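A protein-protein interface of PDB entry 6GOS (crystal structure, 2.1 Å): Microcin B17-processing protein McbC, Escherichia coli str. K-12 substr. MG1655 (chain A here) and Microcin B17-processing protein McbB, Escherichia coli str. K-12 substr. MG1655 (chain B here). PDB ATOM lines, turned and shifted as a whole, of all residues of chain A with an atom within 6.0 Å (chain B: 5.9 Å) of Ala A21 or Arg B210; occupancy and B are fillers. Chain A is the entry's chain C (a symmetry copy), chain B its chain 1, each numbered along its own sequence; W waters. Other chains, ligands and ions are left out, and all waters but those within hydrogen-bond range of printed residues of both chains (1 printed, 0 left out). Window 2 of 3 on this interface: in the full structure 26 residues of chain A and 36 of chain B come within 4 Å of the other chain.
Of the 8 printed residues of chain B, 5 touch a printed residue of chain A. Hydrophobic or aromatic side chains of chain B within 4 Å of the printed part of chain A: Ile B285. Hydrophobic or aromatic side chains of chain A that line the printed part of chain B: Pro A17 and Ala A21. Among the printed residues, Asp or Glu carboxylates within 4 Å of a Lys or Arg side-chain nitrogen of the other chain: Asp A25 with Arg B199 (3.2 Å) and Asp A25 with Arg B210 (2.6 Å).
The backbone carbonyl oxygen of Arg B199 lies within hydrogen-bond range of the side-chain hydroxyl of Ser B202 (2.9 Å). N of Glu A18 lies within hydrogen-bond range of OD1 of Asp A16, 2.9 Å away.
Ala A21 touches just one residue of chain B: Arg B210. Printed residues of chain B within 4 Å of Lys A24: Ile B285 (3.4 Å). Of the printed residues of chain A, Ile B285 touches Lys A24 (3.4 Å) and Asp A25 (3.7 Å). The nearest residue of chain A that does not touch Arg B210 is Ile A22 (4.1 Å).
Water W1 lies within hydrogen-bond range of OD1 of Asp A25 (2.7 Å), NE of Arg B199 (3.0 Å) and N of Ile B285 (3.1 Å).
OD2 of Asp A25 is in salt-bridge range of NH2 of Arg B199. The backbone NH (N) of Arg B210 is in hydrogen-bond range of the side-chain carboxylate (OE2) of Glu A18. The guanidinium group of Arg B210 is in salt-bridge range of the side-chain carboxylate of Asp A25, 2.6 Å away. The backbone NH of Asn B211 is in hydrogen-bond range of the side-chain carboxylate of Glu A18 (2.9 Å).
Among the printed residues, pairs that only touch across the chains: Pro A17 with Asn B211, Glu A18 with Arg B209, Ala A21 with Arg B210, Lys A24 with Ile B285 and Asp A25 with Ile B285.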
ATOM      1  N   ASP A  16      -8.010  -6.440  31.594  1.00  0.00           N
ATOM      2  CA  ASP A  16      -7.253  -6.297  30.363  1.00  0.00           C
ATOM      3  C   ASP A  16      -6.520  -7.619  30.141  1.00  0.00           C
ATOM      4  O   ASP A  16      -5.613  -7.973  30.905  1.00  0.00           O
ATOM      5  CB  ASP A  16      -6.269  -5.140  30.443  1.00  0.00           C
ATOM      6  CG  ASP A  16      -5.492  -4.934  29.119  1.00  0.00           C
ATOM      7  OD1 ASP A  16      -5.326  -5.897  28.333  1.00  0.00           O
ATOM      8  OD2 ASP A  16      -5.049  -3.805  28.853  1.00  0.00           O
ATOM      9  N   PRO A  17      -6.884  -8.347  29.081  1.00  0.00           N
ATOM     10  CA  PRO A  17      -6.275  -9.665  28.891  1.00  0.00           C
ATOM     11  C   PRO A  17      -4.763  -9.641  28.576  1.00  0.00           C
ATOM     12  O   PRO A  17      -4.090 -10.621  28.828  1.00  0.00           O
ATOM     13  CB  PRO A  17      -7.047 -10.237  27.694  1.00  0.00           C
ATOM     14  CG  PRO A  17      -7.458  -9.035  26.924  1.00  0.00           C
ATOM     15  CD  PRO A  17      -7.722  -7.956  27.938  1.00  0.00           C
ATOM     16  N   GLU A  18      -4.264  -8.559  27.995  1.00  0.00           N
ATOM     17  CA  GLU A  18      -2.832  -8.408  27.754  1.00  0.00           C
ATOM     18  C   GLU A  18      -2.082  -8.294  29.104  1.00  0.00           C
ATOM     19  O   GLU A  18      -1.068  -8.965  29.347  1.00  0.00           O
ATOM     20  CB  GLU A  18      -2.580  -7.182  26.859  1.00  0.00           C
ATOM     21  CG  GLU A  18      -1.122  -6.973  26.439  1.00  0.00           C
ATOM     22  CD  GLU A  18      -0.688  -7.796  25.226  1.00  0.00           C
ATOM     23  OE1 GLU A  18      -1.510  -8.547  24.648  1.00  0.00           O
ATOM     24  OE2 GLU A  18       0.498  -7.680  24.834  1.00  0.00           O
ATOM     25  N   VAL A  19      -2.595  -7.458  29.985  1.00  0.00           N
ATOM     26  CA  VAL A  19      -2.000  -7.300  31.306  1.00  0.00           C
ATOM     27  C   VAL A  19      -1.960  -8.646  32.006  1.00  0.00           C
ATOM     28  O   VAL A  19      -0.921  -9.014  32.556  1.00  0.00           O
ATOM     29  CB  VAL A  19      -2.790  -6.301  32.184  1.00  0.00           C
ATOM     30  CG1 VAL A  19      -2.180  -6.206  33.578  1.00  0.00           C
ATOM     31  CG2 VAL A  19      -2.822  -4.924  31.554  1.00  0.00           C
ATOM     32  N   LEU A  20      -3.088  -9.380  31.987  1.00  0.00           N
ATOM     33  CA  LEU A  20      -3.232 -10.625  32.735  1.00  0.00           C
ATOM     34  C   LEU A  20      -2.261 -11.669  32.243  1.00  0.00           C
ATOM     35  O   LEU A  20      -1.639 -12.329  33.053  1.00  0.00           O
ATOM     36  CB  LEU A  20      -4.643 -11.187  32.646  1.00  0.00           C
ATOM     37  CG  LEU A  20      -4.900 -12.511  33.371  1.00  0.00           C
ATOM     38  CD1 LEU A  20      -4.759 -12.355  34.871  1.00  0.00           C
ATOM     39  CD2 LEU A  20      -6.280 -13.024  32.990  1.00  0.00           C
ATOM     40  N   ALA A  21      -2.128 -11.798  30.925  1.00  0.00           N
ATOM     41  CA  ALA A  21      -1.185 -12.753  30.327  1.00  0.00           C
ATOM     42  C   ALA A  21       0.252 -12.412  30.657  1.00  0.00           C
ATOM     43  O   ALA A  21       1.025 -13.315  30.971  1.00  0.00           O
ATOM     44  CB  ALA A  21      -1.339 -12.814  28.819  1.00  0.00           C
ATOM     45  N   ILE A  22       0.617 -11.131  30.556  1.00  0.00           N
ATOM     46  CA  ILE A  22       2.006 -10.711  30.790  1.00  0.00           C
ATOM     47  C   ILE A  22       2.411 -10.906  32.260  1.00  0.00           C
ATOM     48  O   ILE A  22       3.541 -11.348  32.549  1.00  0.00           O
ATOM     49  CB  ILE A  22       2.239  -9.271  30.282  1.00  0.00           C
ATOM     50  CG1 ILE A  22       2.210  -9.290  28.751  1.00  0.00           C
ATOM     51  CG2 ILE A  22       3.549  -8.672  30.817  1.00  0.00           C
ATOM     52  CD1 ILE A  22       2.357  -7.936  28.072  1.00  0.00           C
ATOM     53  N   VAL A  23       1.499 -10.589  33.179  1.00  0.00           N
ATOM     54  CA  VAL A  23       1.715 -10.833  34.612  1.00  0.00           C
ATOM     55  C   VAL A  23       1.872 -12.344  34.958  1.00  0.00           C
ATOM     56  O   VAL A  23       2.776 -12.713  35.701  1.00  0.00           O
ATOM     57  CB  VAL A  23       0.590 -10.212  35.460  1.00  0.00           C
ATOM     58  CG1 VAL A  23       0.687 -10.642  36.919  1.00  0.00           C
ATOM     59  CG2 VAL A  23       0.602  -8.691  35.343  1.00  0.00           C
ATOM     60  N   LYS A  24       0.976 -13.196  34.454  1.00  0.00           N
ATOM     61  CA  LYS A  24       1.102 -14.639  34.656  1.00  0.00           C
ATOM     62  C   LYS A  24       2.406 -15.199  34.090  1.00  0.00           C
ATOM     63  O   LYS A  24       3.060 -16.045  34.705  1.00  0.00           O
ATOM     64  CB  LYS A  24      -0.066 -15.377  34.015  1.00  0.00           C
ATOM     65  CG  LYS A  24      -1.390 -15.282  34.758  1.00  0.00           C
ATOM     66  CD  LYS A  24      -2.461 -15.837  33.822  1.00  0.00           C
ATOM     67  CE  LYS A  24      -3.752 -16.139  34.511  1.00  0.00           C
ATOM     68  NZ  LYS A  24      -4.547 -17.089  33.657  1.00  0.00           N
ATOM     69  N   ASP A  25       2.758 -14.761  32.887  1.00  0.00           N
ATOM     70  CA  ASP A  25       3.982 -15.229  32.230  1.00  0.00           C
ATOM     71  C   ASP A  25       5.184 -14.926  33.094  1.00  0.00           C
ATOM     72  O   ASP A  25       6.115 -15.711  33.134  1.00  0.00           O
ATOM     73  CB  ASP A  25       4.229 -14.507  30.916  1.00  0.00           C
ATOM     74  CG  ASP A  25       3.350 -14.975  29.812  1.00  0.00           C
ATOM     75  OD1 ASP A  25       2.693 -16.046  29.925  1.00  0.00           O
ATOM     76  OD2 ASP A  25       3.345 -14.243  28.795  1.00  0.00           O
ATOM     77  N   PHE A  26       5.175 -13.752  33.716  1.00  0.00           N
ATOM     78  CA  PHE A  26       6.258 -13.353  34.593  1.00  0.00           C
ATOM     79  C   PHE A  26       6.224 -14.140  35.892  1.00  0.00           C
ATOM     80  O   PHE A  26       7.245 -14.653  36.336  1.00  0.00           O
ATOM     81  CB  PHE A  26       6.213 -11.863  34.919  1.00  0.00           C
ATOM     82  CG  PHE A  26       7.260 -11.465  35.921  1.00  0.00           C
ATOM     83  CD1 PHE A  26       8.606 -11.400  35.537  1.00  0.00           C
ATOM     84  CD2 PHE A  26       6.932 -11.236  37.238  1.00  0.00           C
ATOM     85  CE1 PHE A  26       9.591 -11.077  36.455  1.00  0.00           C
ATOM     86  CE2 PHE A  26       7.908 -10.899  38.156  1.00  0.00           C
ATOM     87  CZ  PHE A  26       9.241 -10.821  37.763  1.00  0.00           C
ATOM     88  N   ARG B 199       0.585 -21.587  23.504  1.00  0.00           N
ATOM     89  CA  ARG B 199       1.555 -20.520  23.745  1.00  0.00           C
ATOM     90  C   ARG B 199       2.370 -20.246  22.446  1.00  0.00           C
ATOM     91  O   ARG B 199       2.483 -19.082  22.010  1.00  0.00           O
ATOM     92  CB  ARG B 199       2.477 -20.887  24.916  1.00  0.00           C
ATOM     93  CG  ARG B 199       3.495 -19.835  25.318  1.00  0.00           C
ATOM     94  CD  ARG B 199       2.837 -18.782  26.182  1.00  0.00           C
ATOM     95  NE  ARG B 199       3.765 -17.764  26.663  1.00  0.00           N
ATOM     96  CZ  ARG B 199       4.174 -16.690  25.972  1.00  0.00           C
ATOM     97  NH1 ARG B 199       3.775 -16.452  24.719  1.00  0.00           N
ATOM     98  NH2 ARG B 199       5.020 -15.844  26.542  1.00  0.00           N
ATOM     99  N   SER B 202       0.198 -18.844  19.244  1.00  0.00           N
ATOM    100  CA  SER B 202      -0.166 -17.441  19.391  1.00  0.00           C
ATOM    101  C   SER B 202       1.061 -16.529  19.216  1.00  0.00           C
ATOM    102  O   SER B 202       0.981 -15.535  18.493  1.00  0.00           O
ATOM    103  CB  SER B 202      -0.776 -17.192  20.760  1.00  0.00           C
ATOM    104  OG  SER B 202       0.240 -17.314  21.752  1.00  0.00           O
ATOM    105  N   PHE B 208       1.707  -8.879  17.040  1.00  0.00           N
ATOM    106  CA  PHE B 208       2.402  -8.073  18.082  1.00  0.00           C
ATOM    107  C   PHE B 208       1.776  -8.049  19.500  1.00  0.00           C
ATOM    108  O   PHE B 208       2.085  -7.150  20.297  1.00  0.00           O
ATOM    109  CB  PHE B 208       2.598  -6.621  17.573  1.00  0.00           C
ATOM    110  CG  PHE B 208       3.489  -6.513  16.360  1.00  0.00           C
ATOM    111  CD1 PHE B 208       4.871  -6.358  16.506  1.00  0.00           C
ATOM    112  CD2 PHE B 208       2.951  -6.581  15.067  1.00  0.00           C
ATOM    113  CE1 PHE B 208       5.693  -6.274  15.394  1.00  0.00           C
ATOM    114  CE2 PHE B 208       3.770  -6.498  13.954  1.00  0.00           C
ATOM    115  CZ  PHE B 208       5.144  -6.346  14.121  1.00  0.00           C
ATOM    116  N   ARG B 209       0.919  -9.036  19.800  1.00  0.00           N
ATOM    117  CA  ARG B 209       0.149  -9.086  21.046  1.00  0.00           C
ATOM    118  C   ARG B 209       0.458 -10.412  21.731  1.00  0.00           C
ATOM    119  O   ARG B 209       0.505 -11.460  21.087  1.00  0.00           O
ATOM    120  CB  ARG B 209      -1.379  -8.941  20.809  1.00  0.00           C
ATOM    121  CG  ARG B 209      -1.862  -7.571  20.335  1.00  0.00           C
ATOM    122  CD  ARG B 209      -1.912  -6.508  21.428  1.00  0.00           C
ATOM    123  N   ARG B 210       0.694 -10.349  23.037  1.00  0.00           N
ATOM    124  CA  ARG B 210       0.708 -11.545  23.877  1.00  0.00           C
ATOM    125  C   ARG B 210      -0.683 -12.194  23.929  1.00  0.00           C
ATOM    126  O   ARG B 210      -0.786 -13.399  23.751  1.00  0.00           O
ATOM    127  CB  ARG B 210       1.197 -11.216  25.298  1.00  0.00           C
ATOM    128  CG  ARG B 210       1.139 -12.365  26.297  1.00  0.00           C
ATOM    129  CD  ARG B 210       1.996 -13.537  25.887  1.00  0.00           C
ATOM    130  NE  ARG B 210       1.778 -14.635  26.821  1.00  0.00           N
ATOM    131  CZ  ARG B 210       0.794 -15.523  26.746  1.00  0.00           C
ATOM    132  NH1 ARG B 210      -0.094 -15.481  25.755  1.00  0.00           N
ATOM    133  NH2 ARG B 210       0.692 -16.456  27.686  1.00  0.00           N
ATOM    134  N   ASN B 211      -1.718 -11.398  24.200  1.00  0.00           N
ATOM    135  CA  ASN B 211      -3.092 -11.899  24.213  1.00  0.00           C
ATOM    136  C   ASN B 211      -3.534 -12.451  22.851  1.00  0.00           C
ATOM    137  O   ASN B 211      -3.701 -11.698  21.889  1.00  0.00           O
ATOM    138  CB  ASN B 211      -4.094 -10.826  24.629  1.00  0.00           C
ATOM    139  CG  ASN B 211      -5.515 -11.301  24.472  1.00  0.00           C
ATOM    140  OD1 ASN B 211      -5.869 -12.369  24.964  1.00  0.00           O
ATOM    141  ND2 ASN B 211      -6.319 -10.558  23.723  1.00  0.00           N
ATOM    142  N   GLU B 212      -3.761 -13.765  22.819  1.00  0.00           N
ATOM    143  CA  GLU B 212      -4.172 -14.484  21.613  1.00  0.00           C
ATOM    144  C   GLU B 212      -5.663 -14.302  21.243  1.00  0.00           C
ATOM    145  O   GLU B 212      -6.034 -14.669  20.132  1.00  0.00           O
ATOM    146  CB  GLU B 212      -3.815 -15.997  21.732  1.00  0.00           C
ATOM    147  CG  GLU B 212      -4.832 -16.960  22.398  1.00  0.00           C
ATOM    148  CD  GLU B 212      -4.800 -17.024  23.936  1.00  0.00           C
ATOM    149  OE1 GLU B 212      -3.878 -16.479  24.574  1.00  0.00           O
ATOM    150  OE2 GLU B 212      -5.709 -17.651  24.531  1.00  0.00           O
ATOM    151  N   ILE B 285       2.563 -20.910  31.099  1.00  0.00           N
ATOM    152  CA  ILE B 285       1.374 -20.877  31.936  1.00  0.00           C
ATOM    153  C   ILE B 285       0.312 -21.864  31.438  1.00  0.00           C
ATOM    154  O   ILE B 285       0.354 -22.314  30.285  1.00  0.00           O
ATOM    155  CB  ILE B 285       0.768 -19.463  32.067  1.00  0.00           C
ATOM    156  CG1 ILE B 285       0.317 -18.872  30.708  1.00  0.00           C
ATOM    157  CG2 ILE B 285       1.757 -18.540  32.773  1.00  0.00           C
ATOM    158  CD1 ILE B 285      -0.496 -17.609  30.860  1.00  0.00           C
HETATM  159  O   HOH W   1       3.820 -18.486  29.548  1.00  0.00           O
